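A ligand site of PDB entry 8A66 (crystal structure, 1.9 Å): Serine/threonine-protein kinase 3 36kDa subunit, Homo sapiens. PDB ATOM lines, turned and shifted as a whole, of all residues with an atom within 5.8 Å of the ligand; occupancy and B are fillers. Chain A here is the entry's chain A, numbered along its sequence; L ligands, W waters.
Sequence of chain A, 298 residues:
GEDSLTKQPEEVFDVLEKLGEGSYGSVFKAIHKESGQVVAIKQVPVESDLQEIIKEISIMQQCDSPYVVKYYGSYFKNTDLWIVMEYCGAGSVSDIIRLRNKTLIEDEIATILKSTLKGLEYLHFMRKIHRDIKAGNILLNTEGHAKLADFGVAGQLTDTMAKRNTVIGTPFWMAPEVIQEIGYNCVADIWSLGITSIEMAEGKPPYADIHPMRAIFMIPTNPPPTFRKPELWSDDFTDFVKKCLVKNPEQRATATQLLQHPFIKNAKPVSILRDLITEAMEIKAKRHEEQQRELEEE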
ATOM      1  N   LYS A  18      12.883 -13.406  -2.788  1.00  0.00           N
ATOM      2  CA  LYS A  18      13.814 -13.953  -1.819  1.00  0.00           C
ATOM      3  C   LYS A  18      14.184 -15.350  -2.292  1.00  0.00           C
ATOM      4  O   LYS A  18      13.308 -16.133  -2.616  1.00  0.00           O
ATOM      5  CB  LYS A  18      13.132 -14.046  -0.452  1.00  0.00           C
ATOM      6  CG  LYS A  18      13.998 -14.616   0.649  1.00  0.00           C
ATOM      7  CD  LYS A  18      13.724 -13.881   1.950  1.00  0.00           C
ATOM      8  CE  LYS A  18      14.395 -14.533   3.119  1.00  0.00           C
ATOM      9  NZ  LYS A  18      13.438 -15.259   4.010  1.00  0.00           N
ATOM     10  N   LEU A  19      15.485 -15.630  -2.356  1.00  0.00           N
ATOM     11  CA  LEU A  19      15.974 -16.936  -2.792  1.00  0.00           C
ATOM     12  C   LEU A  19      16.010 -17.920  -1.622  1.00  0.00           C
ATOM     13  O   LEU A  19      16.314 -17.539  -0.475  1.00  0.00           O
ATOM     14  CB  LEU A  19      17.354 -16.779  -3.457  1.00  0.00           C
ATOM     15  CG  LEU A  19      17.325 -16.025  -4.791  1.00  0.00           C
ATOM     16  CD1 LEU A  19      18.734 -15.655  -5.244  1.00  0.00           C
ATOM     17  CD2 LEU A  19      16.578 -16.833  -5.870  1.00  0.00           C
ATOM     18  N   GLY A  20      15.684 -19.178  -1.925  1.00  0.00           N
ATOM     19  CA  GLY A  20      15.640 -20.257  -0.944  1.00  0.00           C
ATOM     20  C   GLY A  20      14.414 -21.130  -1.054  1.00  0.00           C
ATOM     21  O   GLY A  20      13.294 -20.702  -0.736  1.00  0.00           O
ATOM     22  N   VAL A  27      18.863 -13.509   1.155  1.00  0.00           N
ATOM     23  CA  VAL A  27      19.355 -13.346  -0.209  1.00  0.00           C
ATOM     24  C   VAL A  27      18.201 -13.198  -1.190  1.00  0.00           C
ATOM     25  O   VAL A  27      17.208 -13.901  -1.069  1.00  0.00           O
ATOM     26  CB  VAL A  27      20.312 -14.474  -0.624  1.00  0.00           C
ATOM     27  CG1 VAL A  27      20.946 -14.192  -1.974  1.00  0.00           C
ATOM     28  CG2 VAL A  27      21.380 -14.701   0.438  1.00  0.00           C
ATOM     29  N   ALA A  40      22.679 -12.199  -7.128  1.00  0.00           N
ATOM     30  CA  ALA A  40      22.093 -12.588  -5.857  1.00  0.00           C
ATOM     31  C   ALA A  40      22.544 -11.529  -4.846  1.00  0.00           C
ATOM     32  O   ALA A  40      23.744 -11.280  -4.714  1.00  0.00           O
ATOM     33  CB  ALA A  40      22.597 -13.956  -5.430  1.00  0.00           C
ATOM     34  N   LYS A  42      22.487 -10.026  -0.924  1.00  0.00           N
ATOM     35  CA  LYS A  42      22.212 -10.287   0.478  1.00  0.00           C
ATOM     36  C   LYS A  42      21.937  -8.973   1.239  1.00  0.00           C
ATOM     37  O   LYS A  42      22.729  -8.025   1.156  1.00  0.00           O
ATOM     38  CB  LYS A  42      23.366 -11.076   1.125  1.00  0.00           C
ATOM     39  CG  LYS A  42      23.101 -11.430   2.572  1.00  0.00           C
ATOM     40  CD  LYS A  42      23.895 -12.622   3.026  1.00  0.00           C
ATOM     41  CE  LYS A  42      25.314 -12.240   3.302  1.00  0.00           C
ATOM     42  NZ  LYS A  42      26.220 -13.427   3.166  1.00  0.00           N
ATOM     43  N   VAL A  69      31.903 -18.579  -5.124  1.00  0.00           N
ATOM     44  CA  VAL A  69      30.936 -17.534  -5.470  1.00  0.00           C
ATOM     45  C   VAL A  69      31.645 -16.178  -5.512  1.00  0.00           C
ATOM     46  O   VAL A  69      32.471 -15.855  -4.640  1.00  0.00           O
ATOM     47  CB  VAL A  69      29.706 -17.568  -4.522  1.00  0.00           C
ATOM     48  CG1 VAL A  69      28.958 -16.242  -4.492  1.00  0.00           C
ATOM     49  CG2 VAL A  69      28.770 -18.696  -4.895  1.00  0.00           C
ATOM     50  N   MET A  85      26.333 -10.421  -5.224  1.00  0.00           N
ATOM     51  CA  MET A  85      27.100 -11.614  -5.464  1.00  0.00           C
ATOM     52  C   MET A  85      26.606 -12.377  -6.703  1.00  0.00           C
ATOM     53  O   MET A  85      25.549 -12.073  -7.238  1.00  0.00           O
ATOM     54  CB  MET A  85      27.026 -12.521  -4.213  1.00  0.00           C
ATOM     55  CG  MET A  85      27.821 -11.998  -3.034  1.00  0.00           C
ATOM     56  SD  MET A  85      27.375 -12.821  -1.489  1.00  0.00           S
ATOM     57  CE  MET A  85      25.694 -12.309  -1.340  1.00  0.00           C
ATOM     58  N   GLU A  86      27.398 -13.367  -7.129  1.00  0.00           N
ATOM     59  CA  GLU A  86      27.104 -14.237  -8.251  1.00  0.00           C
ATOM     60  C   GLU A  86      25.886 -15.090  -7.948  1.00  0.00           C
ATOM     61  O   GLU A  86      25.812 -15.690  -6.864  1.00  0.00           O
ATOM     62  CB  GLU A  86      28.314 -15.147  -8.464  1.00  0.00           C
ATOM     63  CG  GLU A  86      28.124 -16.207  -9.529  1.00  0.00           C
ATOM     64  CD  GLU A  86      29.241 -17.228  -9.598  1.00  0.00           C
ATOM     65  OE1 GLU A  86      30.300 -17.039  -8.946  1.00  0.00           O
ATOM     66  OE2 GLU A  86      29.051 -18.235 -10.314  1.00  0.00           O
ATOM     67  N   TYR A  87      24.943 -15.160  -8.910  1.00  0.00           N
ATOM     68  CA  TYR A  87      23.722 -15.967  -8.825  1.00  0.00           C
ATOM     69  C   TYR A  87      23.952 -17.369  -9.430  1.00  0.00           C
ATOM     70  O   TYR A  87      24.388 -17.485 -10.573  1.00  0.00           O
ATOM     71  CB  TYR A  87      22.592 -15.270  -9.611  1.00  0.00           C
ATOM     72  CG  TYR A  87      21.299 -16.052  -9.670  1.00  0.00           C
ATOM     73  CD1 TYR A  87      20.450 -16.112  -8.580  1.00  0.00           C
ATOM     74  CD2 TYR A  87      20.914 -16.714 -10.828  1.00  0.00           C
ATOM     75  CE1 TYR A  87      19.255 -16.819  -8.629  1.00  0.00           C
ATOM     76  CE2 TYR A  87      19.706 -17.399 -10.903  1.00  0.00           C
ATOM     77  CZ  TYR A  87      18.881 -17.452  -9.794  1.00  0.00           C
ATOM     78  OH  TYR A  87      17.690 -18.140  -9.843  1.00  0.00           O
ATOM     79  N   CYS A  88      23.638 -18.409  -8.669  1.00  0.00           N
ATOM     80  CA  CYS A  88      23.746 -19.794  -9.129  1.00  0.00           C
ATOM     81  C   CYS A  88      22.299 -20.255  -9.328  1.00  0.00           C
ATOM     82  O   CYS A  88      21.577 -20.403  -8.357  1.00  0.00           O
ATOM     83  CB  CYS A  88      24.456 -20.642  -8.076  1.00  0.00           C
ATOM     84  SG  CYS A  88      26.124 -20.080  -7.648  1.00  0.00           S
ATOM     85  N   GLY A  89      21.881 -20.443 -10.581  1.00  0.00           N
ATOM     86  CA  GLY A  89      20.518 -20.832 -10.954  1.00  0.00           C
ATOM     87  C   GLY A  89      19.853 -22.055 -10.351  1.00  0.00           C
ATOM     88  O   GLY A  89      18.616 -22.062 -10.174  1.00  0.00           O
ATOM     89  N   ALA A  90      20.620 -23.118 -10.040  1.00  0.00           N
ATOM     90  CA  ALA A  90      20.004 -24.328  -9.475  1.00  0.00           C
ATOM     91  C   ALA A  90      19.774 -24.285  -7.953  1.00  0.00           C
ATOM     92  O   ALA A  90      19.063 -25.134  -7.418  1.00  0.00           O
ATOM     93  CB  ALA A  90      20.797 -25.552  -9.874  1.00  0.00           C
ATOM     94  N   GLY A  91      20.312 -23.282  -7.270  1.00  0.00           N
ATOM     95  CA  GLY A  91      20.171 -23.180  -5.823  1.00  0.00           C
ATOM     96  C   GLY A  91      21.194 -24.021  -5.083  1.00  0.00           C
ATOM     97  O   GLY A  91      22.192 -24.454  -5.662  1.00  0.00           O
ATOM     98  N   SER A  92      20.980 -24.219  -3.769  1.00  0.00           N
ATOM     99  CA  SER A  92      21.909 -25.005  -2.971  1.00  0.00           C
ATOM    100  C   SER A  92      21.618 -26.485  -3.114  1.00  0.00           C
ATOM    101  O   SER A  92      20.504 -26.852  -3.554  1.00  0.00           O
ATOM    102  CB  SER A  92      21.870 -24.585  -1.513  1.00  0.00           C
ATOM    103  OG  SER A  92      20.670 -24.953  -0.869  1.00  0.00           O
ATOM    104  N   ASP A  95      18.562 -27.067  -1.176  1.00  0.00           N
ATOM    105  CA  ASP A  95      17.361 -26.634  -1.873  1.00  0.00           C
ATOM    106  C   ASP A  95      16.886 -27.752  -2.806  1.00  0.00           C
ATOM    107  O   ASP A  95      15.708 -28.058  -2.821  1.00  0.00           O
ATOM    108  CB  ASP A  95      17.618 -25.370  -2.722  1.00  0.00           C
ATOM    109  CG  ASP A  95      17.688 -24.050  -1.972  1.00  0.00           C
ATOM    110  OD1 ASP A  95      17.153 -23.969  -0.830  1.00  0.00           O
ATOM    111  OD2 ASP A  95      18.272 -23.089  -2.521  1.00  0.00           O
ATOM    112  N   ARG A  98      15.383 -30.572  -0.861  1.00  0.00           N
ATOM    113  CA  ARG A  98      14.077 -30.150  -0.331  1.00  0.00           C
ATOM    114  C   ARG A  98      12.992 -30.121  -1.477  1.00  0.00           C
ATOM    115  O   ARG A  98      11.952 -30.756  -1.351  1.00  0.00           O
ATOM    116  CB  ARG A  98      14.222 -28.780   0.358  1.00  0.00           C
ATOM    117  CG  ARG A  98      12.909 -28.153   0.832  1.00  0.00           C
ATOM    118  CD  ARG A  98      13.027 -26.648   1.087  1.00  0.00           C
ATOM    119  NE  ARG A  98      12.520 -25.811  -0.017  1.00  0.00           N
ATOM    120  CZ  ARG A  98      13.253 -24.962  -0.716  1.00  0.00           C
ATOM    121  NH1 ARG A  98      12.704 -24.233  -1.686  1.00  0.00           N
ATOM    122  NH2 ARG A  98      14.550 -24.803  -0.452  1.00  0.00           N
ATOM    123  N   LEU A  99      13.290 -29.415  -2.582  1.00  0.00           N
ATOM    124  CA  LEU A  99      12.445 -29.262  -3.762  1.00  0.00           C
ATOM    125  C   LEU A  99      11.935 -30.606  -4.303  1.00  0.00           C
ATOM    126  O   LEU A  99      10.722 -30.802  -4.439  1.00  0.00           O
ATOM    127  CB  LEU A  99      13.266 -28.519  -4.862  1.00  0.00           C
ATOM    128  CG  LEU A  99      13.029 -27.015  -5.169  1.00  0.00           C
ATOM    129  CD1 LEU A  99      12.090 -26.327  -4.189  1.00  0.00           C
ATOM    130  CD2 LEU A  99      14.321 -26.287  -5.382  1.00  0.00           C
ATOM    131  N   GLY A 136      23.697 -26.550   2.455  1.00  0.00           N
ATOM    132  CA  GLY A 136      23.067 -25.239   2.284  1.00  0.00           C
ATOM    133  C   GLY A 136      23.991 -24.200   1.698  1.00  0.00           C
ATOM    134  O   GLY A 136      23.526 -23.190   1.136  1.00  0.00           O
ATOM    135  N   ASN A 137      25.329 -24.400   1.854  1.00  0.00           N
ATOM    136  CA  ASN A 137      26.345 -23.459   1.357  1.00  0.00           C
ATOM    137  C   ASN A 137      27.126 -23.983   0.132  1.00  0.00           C
ATOM    138  O   ASN A 137      28.153 -23.391  -0.250  1.00  0.00           O
ATOM    139  CB  ASN A 137      27.278 -23.027   2.466  1.00  0.00           C
ATOM    140  CG  ASN A 137      26.593 -22.230   3.531  1.00  0.00           C
ATOM    141  OD1 ASN A 137      25.553 -21.611   3.303  1.00  0.00           O
ATOM    142  ND2 ASN A 137      27.169 -22.188   4.724  1.00  0.00           N
ATOM    143  N   LEU A 139      26.451 -24.285  -3.667  1.00  0.00           N
ATOM    144  CA  LEU A 139      25.477 -23.822  -4.650  1.00  0.00           C
ATOM    145  C   LEU A 139      25.782 -24.327  -6.031  1.00  0.00           C
ATOM    146  O   LEU A 139      26.932 -24.352  -6.422  1.00  0.00           O
ATOM    147  CB  LEU A 139      25.466 -22.300  -4.689  1.00  0.00           C
ATOM    148  CG  LEU A 139      25.238 -21.552  -3.376  1.00  0.00           C
ATOM    149  CD1 LEU A 139      25.154 -20.104  -3.639  1.00  0.00           C
ATOM    150  CD2 LEU A 139      23.965 -21.928  -2.727  1.00  0.00           C
ATOM    151  N   ALA A 149      29.896 -21.111  -1.075  1.00  0.00           N
ATOM    152  CA  ALA A 149      29.245 -19.837  -0.798  1.00  0.00           C
ATOM    153  C   ALA A 149      29.107 -19.605   0.703  1.00  0.00           C
ATOM    154  O   ALA A 149      29.244 -20.536   1.491  1.00  0.00           O
ATOM    155  CB  ALA A 149      27.875 -19.803  -1.476  1.00  0.00           C
ATOM    156  N   ASP A 150      28.874 -18.350   1.111  1.00  0.00           N
ATOM    157  CA  ASP A 150      28.722 -17.921   2.485  1.00  0.00           C
ATOM    158  C   ASP A 150      30.040 -17.918   3.246  1.00  0.00           C
ATOM    159  O   ASP A 150      30.346 -18.845   3.993  1.00  0.00           O
ATOM    160  CB  ASP A 150      27.615 -18.660   3.237  1.00  0.00           C
ATOM    161  CG  ASP A 150      27.120 -17.929   4.484  1.00  0.00           C
ATOM    162  OD1 ASP A 150      27.704 -16.876   4.831  1.00  0.00           O
ATOM    163  OD2 ASP A 150      26.175 -18.408   5.119  1.00  0.00           O
ATOM    164  N   ALA A 280      14.299 -30.163  -9.955  1.00  0.00           N
ATOM    165  CA  ALA A 280      14.247 -29.186  -8.874  1.00  0.00           C
ATOM    166  C   ALA A 280      13.772 -27.821  -9.367  1.00  0.00           C
ATOM    167  O   ALA A 280      12.932 -27.203  -8.715  1.00  0.00           O
ATOM    168  CB  ALA A 280      15.612 -29.067  -8.205  1.00  0.00           C
ATOM    169  N   MET A 281      14.270 -27.369 -10.523  1.00  0.00           N
ATOM    170  CA  MET A 281      13.878 -26.077 -11.095  1.00  0.00           C
ATOM    171  C   MET A 281      12.405 -26.072 -11.553  1.00  0.00           C
ATOM    172  O   MET A 281      11.725 -25.064 -11.390  1.00  0.00           O
ATOM    173  CB  MET A 281      14.785 -25.701 -12.264  1.00  0.00           C
ATOM    174  CG  MET A 281      16.111 -25.114 -11.866  1.00  0.00           C
ATOM    175  SD  MET A 281      16.995 -24.625 -13.384  1.00  0.00           S
ATOM    176  CE  MET A 281      18.524 -24.309 -12.770  1.00  0.00           C
ATOM    177  N   LYS A 284      10.204 -25.795  -8.450  1.00  0.00           N
ATOM    178  CA  LYS A 284      10.276 -24.430  -7.954  1.00  0.00           C
ATOM    179  C   LYS A 284       9.343 -23.521  -8.769  1.00  0.00           C
ATOM    180  O   LYS A 284       8.576 -22.771  -8.190  1.00  0.00           O
ATOM    181  CB  LYS A 284      11.715 -23.891  -8.007  1.00  0.00           C
ATOM    182  CG  LYS A 284      12.181 -23.297  -6.695  1.00  0.00           C
ATOM    183  CD  LYS A 284      11.476 -22.006  -6.321  1.00  0.00           C
ATOM    184  CE  LYS A 284      11.248 -21.931  -4.826  1.00  0.00           C
ATOM    185  NZ  LYS A 284      12.022 -20.824  -4.193  1.00  0.00           N
HETATM  186  C1  LIG L   1      22.170 -17.671  -2.972  1.00  0.00           C
HETATM  187  C2  LIG L   1      23.453 -17.270  -3.458  1.00  0.00           C
HETATM  188  C3  LIG L   1      23.709 -17.463  -4.811  1.00  0.00           C
HETATM  189  N1  LIG L   1      22.815 -18.009  -5.650  1.00  0.00           N
HETATM  190  N2  LIG L   1      21.271 -18.195  -3.832  1.00  0.00           N
HETATM  191  C4  LIG L   1      25.127 -15.459  -3.208  1.00  0.00           C
HETATM  192  N3  LIG L   1      24.522 -16.699  -2.723  1.00  0.00           N
HETATM  193  C5  LIG L   1      24.936 -17.108  -1.484  1.00  0.00           C
HETATM  194  O1  LIG L   1      25.966 -16.678  -0.964  1.00  0.00           O
HETATM  195  C6  LIG L   1      24.134 -18.070  -0.698  1.00  0.00           C
HETATM  196  S1  LIG L   1      24.968 -19.011   0.484  1.00  0.00           S
HETATM  197  C7  LIG L   1      23.494 -19.737   1.016  1.00  0.00           C
HETATM  198  C8  LIG L   1      22.393 -19.281   0.347  1.00  0.00           C
HETATM  199  C9  LIG L   1      22.761 -18.325  -0.648  1.00  0.00           C
HETATM  200  N4  LIG L   1      21.790 -17.933  -1.633  1.00  0.00           N
HETATM  201  C10 LIG L   1      20.379 -18.157  -1.316  1.00  0.00           C
HETATM  202  C11 LIG L   1      21.645 -18.369  -5.100  1.00  0.00           C
HETATM  203  N5  LIG L   1      20.815 -19.047  -5.948  1.00  0.00           N
HETATM  204  C12 LIG L   1      19.542 -19.664  -5.811  1.00  0.00           C
HETATM  205  C13 LIG L   1      18.839 -20.093  -6.923  1.00  0.00           C
HETATM  206  C14 LIG L   1      17.642 -20.774  -6.780  1.00  0.00           C
HETATM  207  C15 LIG L   1      17.156 -21.038  -5.504  1.00  0.00           C
HETATM  208  S2  LIG L   1      15.636 -21.921  -5.308  1.00  0.00           S
HETATM  209  O2  LIG L   1      15.803 -22.854  -4.231  1.00  0.00           O
HETATM  210  O3  LIG L   1      14.584 -20.963  -5.204  1.00  0.00           O
HETATM  211  N6  LIG L   1      15.399 -22.785  -6.647  1.00  0.00           N
HETATM  212  C16 LIG L   1      17.848 -20.598  -4.377  1.00  0.00           C
HETATM  213  C17 LIG L   1      19.036 -19.915  -4.541  1.00  0.00           C
HETATM  214  O   HOH W   1      28.681 -16.128  -0.806  1.00  0.00           O
HETATM  215  O   HOH W   2      25.971 -15.638   1.420  1.00  0.00           O
HETATM  216  O   HOH W   3      19.451 -21.226  -0.580  1.00  0.00           O
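Water W2 lies within hydrogen-bond range of O1 of the ligand (2.6 Å) and NZ of Lys 42 (2.8 Å). Water W1 lies within hydrogen-bond range of an oxygen (O1) of the ligand, the backbone NH (N) of Asp 150 and the side-chain sulfur (SD) of Met 85.
The side-chain amino group (NZ) of Lys 284 sits at hydrogen-bond distance from an oxygen (O3) of the ligand, 2.8 Å away. The backbone NH of Cys 88 is in hydrogen-bond range of a nitrogen (N1) of the ligand, at 3.2 Å. A nitrogen (N5) of the ligand is in hydrogen-bond range of the backbone carbonyl oxygen (O) of Cys 88, at 2.9 Å.
The guanidinium group (NH2) of Arg 98 is in salt-bridge range of the side-chain carboxylate (OD1) of Asp 95, at 2.8 Å. The backbone NH (N) of Asp 95 lies within hydrogen-bond range of the side-chain hydroxyl (OG) of Ser 92, 3.0 Å away. The backbone NH of Ala 149 is in hydrogen-bond range of the backbone carbonyl oxygen of Asn 137. N of Met 85 sits at hydrogen-bond distance from O of Ala 40. The backbone NH (N) of Leu 19 sits at hydrogen-bond distance from the backbone carbonyl oxygen (O) of Val 27 (2.8 Å).
OD2 of Asp 95 lies close to O2 of the ligand (3.0 Å). Residues that only touch the ligand: Leu 139 (3.2 Å), Glu 86 (3.4 Å), Gly 136 (3.5 Å), Gly 91 (3.5 Å), Gly 20 (3.6 Å), Ala 149 (3.6 Å), Asn 137 (3.6 Å), Met 85 (3.6 Å), Ala 40 (3.7 Å), Tyr 87 (3.7 Å), Leu 19 (3.7 Å), Val 27 (3.7 Å), Gly 89 (3.8 Å), Asp 150 (3.8 Å) and Leu 99 (3.9 Å). Hydrophobic or aromatic side chains that line the ligand: Leu 19, Val 27, Ala 40, Met 85, Tyr 87, Leu 99, Leu 139 and Ala 149. Within 4 Å of the ligand: Leu 19, Gly 20, Val 27, Ala 40, Met 85, Glu 86, Tyr 87, Cys 88, Gly 89, Gly 91, Asp 95, Leu 99, Gly 136, Asn 137, Leu 139, Ala 149, Asp 150 and Lys 284.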
